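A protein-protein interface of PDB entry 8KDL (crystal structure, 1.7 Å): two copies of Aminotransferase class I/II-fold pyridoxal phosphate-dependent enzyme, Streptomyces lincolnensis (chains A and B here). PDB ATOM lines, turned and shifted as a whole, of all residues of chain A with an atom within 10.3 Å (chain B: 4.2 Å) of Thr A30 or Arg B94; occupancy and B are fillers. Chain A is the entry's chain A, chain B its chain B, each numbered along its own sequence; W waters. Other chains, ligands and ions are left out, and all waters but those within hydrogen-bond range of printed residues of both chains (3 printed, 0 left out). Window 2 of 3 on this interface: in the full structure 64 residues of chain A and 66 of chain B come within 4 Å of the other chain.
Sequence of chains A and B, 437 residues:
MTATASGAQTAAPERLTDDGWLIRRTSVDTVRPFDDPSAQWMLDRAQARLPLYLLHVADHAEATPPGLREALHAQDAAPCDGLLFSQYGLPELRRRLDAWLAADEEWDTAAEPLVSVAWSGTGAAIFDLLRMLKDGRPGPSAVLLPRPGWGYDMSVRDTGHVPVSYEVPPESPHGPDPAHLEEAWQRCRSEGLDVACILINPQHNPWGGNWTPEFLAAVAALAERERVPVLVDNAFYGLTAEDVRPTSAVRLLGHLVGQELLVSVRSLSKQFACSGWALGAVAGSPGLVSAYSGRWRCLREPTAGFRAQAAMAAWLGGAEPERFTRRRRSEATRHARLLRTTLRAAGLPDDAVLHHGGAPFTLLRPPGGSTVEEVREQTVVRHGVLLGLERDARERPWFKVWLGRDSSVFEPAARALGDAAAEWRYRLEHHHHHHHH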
ATOM      1  N   ARG A  24      10.776   5.138 -28.009  1.00  0.00           N
ATOM      2  CA  ARG A  24      10.073   4.611 -26.844  1.00  0.00           C
ATOM      3  C   ARG A  24      10.611   3.244 -26.441  1.00  0.00           C
ATOM      4  O   ARG A  24      10.683   2.935 -25.243  1.00  0.00           O
ATOM      5  CB  ARG A  24       8.578   4.539 -27.116  1.00  0.00           C
ATOM      6  CG  ARG A  24       7.919   5.930 -27.262  1.00  0.00           C
ATOM      7  CD  ARG A  24       6.398   5.784 -27.213  1.00  0.00           C
ATOM      8  NE  ARG A  24       5.893   5.190 -28.447  1.00  0.00           N
ATOM      9  CZ  ARG A  24       5.732   5.846 -29.590  1.00  0.00           C
ATOM     10  NH1 ARG A  24       5.971   7.142 -29.680  1.00  0.00           N
ATOM     11  NH2 ARG A  24       5.347   5.175 -30.674  1.00  0.00           N
ATOM     12  N   ARG A  25      11.026   2.425 -27.416  1.00  0.00           N
ATOM     13  CA  ARG A  25      11.558   1.115 -27.058  1.00  0.00           C
ATOM     14  C   ARG A  25      13.031   1.182 -26.662  1.00  0.00           C
ATOM     15  O   ARG A  25      13.451   0.474 -25.741  1.00  0.00           O
ATOM     16  CB  ARG A  25      11.382   0.110 -28.205  1.00  0.00           C
ATOM     17  CG  ARG A  25      11.762  -1.299 -27.780  1.00  0.00           C
ATOM     18  CD  ARG A  25      11.443  -2.315 -28.848  1.00  0.00           C
ATOM     19  NE  ARG A  25      11.672  -3.669 -28.358  1.00  0.00           N
ATOM     20  CZ  ARG A  25      11.517  -4.755 -29.103  1.00  0.00           C
ATOM     21  NH1 ARG A  25      11.185  -4.665 -30.384  1.00  0.00           N
ATOM     22  NH2 ARG A  25      11.681  -5.960 -28.541  1.00  0.00           N
ATOM     23  N   THR A  26      13.846   1.997 -27.336  1.00  0.00           N
ATOM     24  CA  THR A  26      15.285   1.856 -27.148  1.00  0.00           C
ATOM     25  C   THR A  26      15.935   2.979 -26.355  1.00  0.00           C
ATOM     26  O   THR A  26      17.124   2.864 -26.040  1.00  0.00           O
ATOM     27  CB  THR A  26      16.030   1.711 -28.494  1.00  0.00           C
ATOM     28  OG1 THR A  26      16.123   2.975 -29.176  1.00  0.00           O
ATOM     29  CG2 THR A  26      15.388   0.642 -29.392  1.00  0.00           C
ATOM     30  N   SER A  27      15.211   4.053 -26.033  1.00  0.00           N
ATOM     31  CA  SER A  27      15.782   5.158 -25.272  1.00  0.00           C
ATOM     32  C   SER A  27      15.165   5.342 -23.898  1.00  0.00           C
ATOM     33  O   SER A  27      15.804   5.950 -23.035  1.00  0.00           O
ATOM     34  CB  SER A  27      15.602   6.485 -26.015  1.00  0.00           C
ATOM     35  OG  SER A  27      16.249   6.455 -27.255  1.00  0.00           O
ATOM     36  N   VAL A  28      13.929   4.897 -23.698  1.00  0.00           N
ATOM     37  CA  VAL A  28      13.230   5.083 -22.429  1.00  0.00           C
ATOM     38  C   VAL A  28      13.782   4.097 -21.412  1.00  0.00           C
ATOM     39  O   VAL A  28      13.744   2.878 -21.621  1.00  0.00           O
ATOM     40  CB  VAL A  28      11.715   4.911 -22.602  1.00  0.00           C
ATOM     41  CG1 VAL A  28      11.025   4.876 -21.250  1.00  0.00           C
ATOM     42  CG2 VAL A  28      11.157   6.042 -23.454  1.00  0.00           C
ATOM     43  N   ASP A  29      14.298   4.621 -20.306  1.00  0.00           N
ATOM     44  CA  ASP A  29      14.985   3.767 -19.351  1.00  0.00           C
ATOM     45  C   ASP A  29      15.114   4.566 -18.059  1.00  0.00           C
ATOM     46  O   ASP A  29      14.767   5.751 -18.005  1.00  0.00           O
ATOM     47  CB  ASP A  29      16.328   3.316 -19.953  1.00  0.00           C
ATOM     48  CG  ASP A  29      16.940   2.102 -19.262  1.00  0.00           C
ATOM     49  OD1 ASP A  29      16.422   1.612 -18.241  1.00  0.00           O
ATOM     50  OD2 ASP A  29      17.891   1.539 -19.867  1.00  0.00           O
ATOM     51  N   THR A  30      15.552   3.892 -17.003  1.00  0.00           N
ATOM     52  CA  THR A  30      15.739   4.556 -15.717  1.00  0.00           C
ATOM     53  C   THR A  30      17.097   5.234 -15.612  1.00  0.00           C
ATOM     54  O   THR A  30      17.440   5.769 -14.549  1.00  0.00           O
ATOM     55  CB  THR A  30      15.535   3.558 -14.572  1.00  0.00           C
ATOM     56  OG1 THR A  30      16.423   2.440 -14.729  1.00  0.00           O
ATOM     57  CG2 THR A  30      14.107   3.068 -14.559  1.00  0.00           C
ATOM     58  N   VAL A  31      17.861   5.229 -16.702  1.00  0.00           N
ATOM     59  CA  VAL A  31      19.096   5.982 -16.828  1.00  0.00           C
ATOM     60  C   VAL A  31      18.982   6.847 -18.073  1.00  0.00           C
ATOM     61  O   VAL A  31      18.209   6.545 -18.987  1.00  0.00           O
ATOM     62  CB  VAL A  31      20.321   5.049 -16.908  1.00  0.00           C
ATOM     63  CG1 VAL A  31      20.443   4.241 -15.618  1.00  0.00           C
ATOM     64  CG2 VAL A  31      20.231   4.133 -18.109  1.00  0.00           C
ATOM     65  N   ARG A  32      19.724   7.951 -18.082  1.00  0.00           N
ATOM     66  CA  ARG A  32      19.788   8.818 -19.252  1.00  0.00           C
ATOM     67  C   ARG A  32      20.435   8.055 -20.411  1.00  0.00           C
ATOM     68  O   ARG A  32      21.533   7.507 -20.248  1.00  0.00           O
ATOM     69  CB  ARG A  32      20.607  10.061 -18.898  1.00  0.00           C
ATOM     70  CG  ARG A  32      20.511  11.215 -19.851  1.00  0.00           C
ATOM     71  CD  ARG A  32      19.523  12.249 -19.334  1.00  0.00           C
ATOM     72  NE  ARG A  32      20.187  13.269 -18.529  1.00  0.00           N
ATOM     73  CZ  ARG A  32      19.567  14.292 -17.956  1.00  0.00           C
ATOM     74  NH1 ARG A  32      18.263  14.473 -18.090  1.00  0.00           N
ATOM     75  NH2 ARG A  32      20.274  15.163 -17.242  1.00  0.00           N
ATOM     76  N   PRO A  33      19.804   7.988 -21.588  1.00  0.00           N
ATOM     77  CA  PRO A  33      20.342   7.090 -22.626  1.00  0.00           C
ATOM     78  C   PRO A  33      21.641   7.579 -23.245  1.00  0.00           C
ATOM     79  O   PRO A  33      22.453   6.750 -23.660  1.00  0.00           O
ATOM     80  CB  PRO A  33      19.200   7.013 -23.649  1.00  0.00           C
ATOM     81  CG  PRO A  33      18.483   8.303 -23.494  1.00  0.00           C
ATOM     82  CD  PRO A  33      18.543   8.623 -22.016  1.00  0.00           C
ATOM     83  N   PHE A  34      21.854   8.888 -23.336  1.00  0.00           N
ATOM     84  CA  PHE A  34      23.151   9.485 -23.636  1.00  0.00           C
ATOM     85  C   PHE A  34      23.002  10.966 -23.339  1.00  0.00           C
ATOM     86  O   PHE A  34      21.886  11.461 -23.200  1.00  0.00           O
ATOM     87  CB  PHE A  34      23.622   9.213 -25.078  1.00  0.00           C
ATOM     88  CG  PHE A  34      22.594   9.486 -26.137  1.00  0.00           C
ATOM     89  CD1 PHE A  34      21.595   8.554 -26.414  1.00  0.00           C
ATOM     90  CD2 PHE A  34      22.665  10.630 -26.918  1.00  0.00           C
ATOM     91  CE1 PHE A  34      20.649   8.796 -27.407  1.00  0.00           C
ATOM     92  CE2 PHE A  34      21.725  10.877 -27.914  1.00  0.00           C
ATOM     93  CZ  PHE A  34      20.718   9.958 -28.158  1.00  0.00           C
ATOM     94  N   LEU A  43      13.308  11.894 -26.772  1.00  0.00           N
ATOM     95  CA  LEU A  43      12.450  11.308 -25.740  1.00  0.00           C
ATOM     96  C   LEU A  43      11.153  12.086 -25.560  1.00  0.00           C
ATOM     97  O   LEU A  43      10.068  11.495 -25.510  1.00  0.00           O
ATOM     98  CB  LEU A  43      13.198  11.222 -24.411  1.00  0.00           C
ATOM     99  CG  LEU A  43      14.225  10.111 -24.241  1.00  0.00           C
ATOM    100  CD1 LEU A  43      15.058  10.336 -22.997  1.00  0.00           C
ATOM    101  CD2 LEU A  43      13.425   8.818 -24.102  1.00  0.00           C
ATOM    102  N   GLN A  47       7.792  10.279 -26.271  1.00  0.00           N
ATOM    103  CA  GLN A  47       6.965   9.921 -25.128  1.00  0.00           C
ATOM    104  C   GLN A  47       5.622  10.631 -25.170  1.00  0.00           C
ATOM    105  O   GLN A  47       4.647  10.118 -24.606  1.00  0.00           O
ATOM    106  CB  GLN A  47       7.720  10.211 -23.835  1.00  0.00           C
ATOM    107  CG  GLN A  47       8.817   9.180 -23.615  1.00  0.00           C
ATOM    108  CD  GLN A  47       9.398   9.217 -22.228  1.00  0.00           C
ATOM    109  OE1 GLN A  47      10.117  10.151 -21.867  1.00  0.00           O
ATOM    110  NE2 GLN A  47       9.074   8.205 -21.429  1.00  0.00           N
ATOM    111  N   TYR B  88      23.751   2.375 -23.369  1.00  0.00           N
ATOM    112  CA  TYR B  88      23.787   1.277 -22.421  1.00  0.00           C
ATOM    113  C   TYR B  88      23.190  -0.013 -22.971  1.00  0.00           C
ATOM    114  O   TYR B  88      23.132  -1.011 -22.238  1.00  0.00           O
ATOM    115  CB  TYR B  88      23.038   1.679 -21.150  1.00  0.00           C
ATOM    116  CG  TYR B  88      23.651   2.855 -20.428  1.00  0.00           C
ATOM    117  CD1 TYR B  88      24.849   2.723 -19.750  1.00  0.00           C
ATOM    118  CD2 TYR B  88      23.045   4.104 -20.452  1.00  0.00           C
ATOM    119  CE1 TYR B  88      25.425   3.802 -19.089  1.00  0.00           C
ATOM    120  CE2 TYR B  88      23.614   5.192 -19.803  1.00  0.00           C
ATOM    121  CZ  TYR B  88      24.807   5.029 -19.124  1.00  0.00           C
ATOM    122  OH  TYR B  88      25.386   6.099 -18.460  1.00  0.00           O
ATOM    123  N   LEU B  90      19.888  -2.107 -25.136  1.00  0.00           N
ATOM    124  CA  LEU B  90      18.420  -2.120 -25.190  1.00  0.00           C
ATOM    125  C   LEU B  90      17.820  -2.115 -23.789  1.00  0.00           C
ATOM    126  O   LEU B  90      18.134  -3.003 -22.994  1.00  0.00           O
ATOM    127  CB  LEU B  90      17.973  -3.359 -25.954  1.00  0.00           C
ATOM    128  CG  LEU B  90      16.477  -3.423 -26.258  1.00  0.00           C
ATOM    129  CD1 LEU B  90      16.047  -2.306 -27.208  1.00  0.00           C
ATOM    130  CD2 LEU B  90      16.156  -4.804 -26.841  1.00  0.00           C
ATOM    131  N   PRO B  91      16.968  -1.144 -23.439  1.00  0.00           N
ATOM    132  CA  PRO B  91      16.525  -1.058 -22.034  1.00  0.00           C
ATOM    133  C   PRO B  91      15.840  -2.320 -21.512  1.00  0.00           C
ATOM    134  O   PRO B  91      16.062  -2.678 -20.355  1.00  0.00           O
ATOM    135  CB  PRO B  91      15.601   0.180 -22.018  1.00  0.00           C
ATOM    136  CG  PRO B  91      15.560   0.677 -23.423  1.00  0.00           C
ATOM    137  CD  PRO B  91      16.716   0.108 -24.166  1.00  0.00           C
ATOM    138  N   GLU B  92      15.056  -3.043 -22.325  1.00  0.00           N
ATOM    139  CA  GLU B  92      14.393  -4.227 -21.777  1.00  0.00           C
ATOM    140  C   GLU B  92      15.405  -5.302 -21.383  1.00  0.00           C
ATOM    141  O   GLU B  92      15.155  -6.071 -20.447  1.00  0.00           O
ATOM    142  CB  GLU B  92      13.366  -4.798 -22.772  1.00  0.00           C
ATOM    143  CG  GLU B  92      13.922  -5.031 -24.157  1.00  0.00           C
ATOM    144  CD  GLU B  92      12.849  -5.069 -25.230  1.00  0.00           C
ATOM    145  OE1 GLU B  92      12.428  -3.979 -25.639  1.00  0.00           O
ATOM    146  OE2 GLU B  92      12.506  -6.154 -25.744  1.00  0.00           O
ATOM    147  N   LEU B  93      16.554  -5.365 -22.074  1.00  0.00           N
ATOM    148  CA  LEU B  93      17.640  -6.258 -21.674  1.00  0.00           C
ATOM    149  C   LEU B  93      18.400  -5.701 -20.477  1.00  0.00           C
ATOM    150  O   LEU B  93      18.706  -6.431 -19.525  1.00  0.00           O
ATOM    151  CB  LEU B  93      18.624  -6.459 -22.830  1.00  0.00           C
ATOM    152  CG  LEU B  93      19.759  -7.434 -22.456  1.00  0.00           C
ATOM    153  CD1 LEU B  93      19.249  -8.736 -21.808  1.00  0.00           C
ATOM    154  CD2 LEU B  93      20.685  -7.736 -23.637  1.00  0.00           C
ATOM    155  N   ARG B  94      18.723  -4.409 -20.524  1.00  0.00           N
ATOM    156  CA  ARG B  94      19.542  -3.826 -19.469  1.00  0.00           C
ATOM    157  C   ARG B  94      18.853  -3.968 -18.114  1.00  0.00           C
ATOM    158  O   ARG B  94      19.484  -4.343 -17.120  1.00  0.00           O
ATOM    159  CB  ARG B  94      19.830  -2.357 -19.796  1.00  0.00           C
ATOM    160  CG  ARG B  94      20.892  -1.733 -18.906  1.00  0.00           C
ATOM    161  CD  ARG B  94      20.849  -0.222 -19.052  1.00  0.00           C
ATOM    162  NE  ARG B  94      19.758   0.344 -18.263  1.00  0.00           N
ATOM    163  CZ  ARG B  94      19.681   0.341 -16.935  1.00  0.00           C
ATOM    164  NH1 ARG B  94      20.677  -0.100 -16.177  1.00  0.00           N
ATOM    165  NH2 ARG B  94      18.583   0.805 -16.350  1.00  0.00           N
ATOM    166  N   ARG B  95      17.546  -3.708 -18.054  1.00  0.00           N
ATOM    167  CA  ARG B  95      16.883  -3.805 -16.763  1.00  0.00           C
ATOM    168  C   ARG B  95      16.707  -5.256 -16.335  1.00  0.00           C
ATOM    169  O   ARG B  95      16.737  -5.543 -15.135  1.00  0.00           O
ATOM    170  CB  ARG B  95      15.563  -3.039 -16.796  1.00  0.00           C
ATOM    171  CG  ARG B  95      14.409  -3.785 -17.332  1.00  0.00           C
ATOM    172  CD  ARG B  95      13.089  -3.058 -17.041  1.00  0.00           C
ATOM    173  NE  ARG B  95      12.152  -3.446 -18.078  1.00  0.00           N
ATOM    174  CZ  ARG B  95      12.018  -2.815 -19.234  1.00  0.00           C
ATOM    175  NH1 ARG B  95      12.630  -1.662 -19.466  1.00  0.00           N
ATOM    176  NH2 ARG B  95      11.249  -3.351 -20.179  1.00  0.00           N
ATOM    177  N   ARG B  96      16.595  -6.188 -17.295  1.00  0.00           N
ATOM    178  CA  ARG B  96      16.585  -7.602 -16.947  1.00  0.00           C
ATOM    179  C   ARG B  96      17.903  -8.016 -16.320  1.00  0.00           C
ATOM    180  O   ARG B  96      17.917  -8.773 -15.345  1.00  0.00           O
ATOM    181  CB  ARG B  96      16.318  -8.472 -18.181  1.00  0.00           C
ATOM    182  CG  ARG B  96      16.145  -9.965 -17.847  1.00  0.00           C
ATOM    183  CD  ARG B  96      14.985 -10.171 -16.835  1.00  0.00           C
ATOM    184  NE  ARG B  96      13.883  -9.256 -17.113  1.00  0.00           N
ATOM    185  CZ  ARG B  96      13.171  -8.609 -16.197  1.00  0.00           C
ATOM    186  NH1 ARG B  96      13.331  -8.836 -14.903  1.00  0.00           N
ATOM    187  NH2 ARG B  96      12.284  -7.698 -16.592  1.00  0.00           N
ATOM    188  N   LEU B  97      19.025  -7.560 -16.891  1.00  0.00           N
ATOM    189  CA  LEU B  97      20.335  -7.921 -16.351  1.00  0.00           C
ATOM    190  C   LEU B  97      20.543  -7.325 -14.964  1.00  0.00           C
ATOM    191  O   LEU B  97      21.124  -7.975 -14.087  1.00  0.00           O
ATOM    192  CB  LEU B  97      21.444  -7.464 -17.305  1.00  0.00           C
ATOM    193  CG  LEU B  97      21.517  -8.222 -18.630  1.00  0.00           C
ATOM    194  CD1 LEU B  97      22.488  -7.537 -19.579  1.00  0.00           C
ATOM    195  CD2 LEU B  97      21.927  -9.648 -18.400  1.00  0.00           C
ATOM    196  N   ASP B  98      20.065  -6.098 -14.749  1.00  0.00           N
ATOM    197  CA  ASP B  98      20.178  -5.468 -13.437  1.00  0.00           C
ATOM    198  C   ASP B  98      19.504  -6.322 -12.369  1.00  0.00           C
ATOM    199  O   ASP B  98      20.114  -6.668 -11.346  1.00  0.00           O
ATOM    200  CB  ASP B  98      19.570  -4.065 -13.484  1.00  0.00           C
ATOM    201  CG  ASP B  98      19.761  -3.299 -12.185  1.00  0.00           C
ATOM    202  OD1 ASP B  98      19.060  -3.622 -11.208  1.00  0.00           O
ATOM    203  OD2 ASP B  98      20.597  -2.373 -12.141  1.00  0.00           O
ATOM    204  N   VAL B 115      24.345  -0.796 -14.458  1.00  0.00           N
ATOM    205  CA  VAL B 115      24.490  -1.983 -15.302  1.00  0.00           C
ATOM    206  C   VAL B 115      24.315  -1.577 -16.763  1.00  0.00           C
ATOM    207  O   VAL B 115      23.385  -0.832 -17.102  1.00  0.00           O
ATOM    208  CB  VAL B 115      23.487  -3.080 -14.891  1.00  0.00           C
ATOM    209  CG1 VAL B 115      23.519  -4.228 -15.880  1.00  0.00           C
ATOM    210  CG2 VAL B 115      23.817  -3.578 -13.476  1.00  0.00           C
ATOM    211  N   VAL B 117      24.811  -3.045 -21.071  1.00  0.00           N
ATOM    212  CA  VAL B 117      24.975  -4.219 -21.931  1.00  0.00           C
ATOM    213  C   VAL B 117      26.292  -4.105 -22.695  1.00  0.00           C
ATOM    214  O   VAL B 117      26.636  -3.040 -23.220  1.00  0.00           O
ATOM    215  CB  VAL B 117      23.799  -4.363 -22.912  1.00  0.00           C
ATOM    216  CG1 VAL B 117      23.959  -5.637 -23.770  1.00  0.00           C
ATOM    217  CG2 VAL B 117      22.455  -4.390 -22.156  1.00  0.00           C
HETATM  218  O   HOH W   1      14.160   0.216 -17.663  1.00  0.00           O
HETATM  219  O   HOH W   2      23.689   8.139 -18.552  1.00  0.00           O
HETATM  220  O   HOH W   3      13.397  -1.900 -24.405  1.00  0.00           O
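No position is printed for both chains.
Water W3 lies within hydrogen-bond range of OE1 of Glu B92 and O of Arg A25. Water W2 lies within hydrogen-bond range of OH of Tyr B88 (2.7 Å) and O of Arg A32 (2.8 Å). Water W1 lies within hydrogen-bond range of OD1 of Asp A29 (2.7 Å) and NH1 of Arg B95 (3.0 Å).
The guanidinium group (NH1) of Arg B94 sits at hydrogen-bond distance from the backbone carbonyl oxygen (O) of Val B115 (3.0 Å). The backbone NH (N) of Val B117 sits at hydrogen-bond distance from the backbone carbonyl oxygen (O) of Tyr B88, at 2.9 Å.
Among the printed residues, pairs that only touch across the chains: Arg A25 with Pro B91 (3.1 Å), Thr A26 with Leu B90 (3.7 Å), Thr A26 with Pro B91 (3.4 Å), Val A28 with Pro B91 (3.3 Å), Asp A29 with Pro B91 (3.4 Å), Val A31 with Tyr B88 (3.7 Å), Val A31 with Arg B94 (3.8 Å) and Arg A32 with Tyr B88 (3.1 Å).
The side-chain carboxylate (OE1) of Glu B92 lies within salt-bridge range of the guanidinium group (NE) of Arg A25 (2.8 Å). OG1 of Thr A30 sits at hydrogen-bond distance from NH2 of Arg B94 (3.2 Å). The guanidinium group (NE) of Arg B94 lies within salt-bridge range of the side-chain carboxylate (OD2) of Asp A29, 2.7 Å away.
Hydrophobic or aromatic side chains of chain A that line the printed part of chain B: Val A31. Of the 12 printed residues of chain B, 5 touch a printed residue of chain A. Hydrophobic or aromatic side chains of chain B that line the printed part of chain A: Tyr B88, Leu B90 and Pro B91. Along chain B the printed residues that touch a printed residue of chain A span positions 88 to 94. Among the printed residues, 11 pairs touch across the chains. Among the printed residues, Asp or Glu carboxylates within 4 Å of a Lys or Arg side-chain nitrogen of the other chain: Arg A25 with Glu B92 (2.8 Å) and Asp A29 with Arg B94 (2.7 Å).
Printed residues of chain B within 4 Å of Thr A26: Leu B90 (3.7 Å) and Pro B91 (3.4 Å). Thr A30 touches just one residue of chain B: Arg B94 (3.2 Å). Of the printed residues of chain B, Val A31 touches Tyr B88 (3.7 Å) and Arg B94 (3.8 Å). Printed residues of chain B within 4 Å of Arg A32: Tyr B88. Printed residues of chain A within 4 Å of Pro B91: Arg A25, Thr A26, Val A28 and Asp A29. No residue of chain A comes within 4 Å of Leu B93. Of the printed residues of chain A, Arg B94 touches Asp A29, Thr A30 and Val A31. Leu B97 touches none of the printed residues of chain A. No residue of chain A comes within 4 Å of Val B115. The nearest printed residue of chain B that does not touch Thr A30 is Arg B95 (5.9 Å). The nearest residue of chain A that does not touch Arg B94 is Val A28 (7.3 Å).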
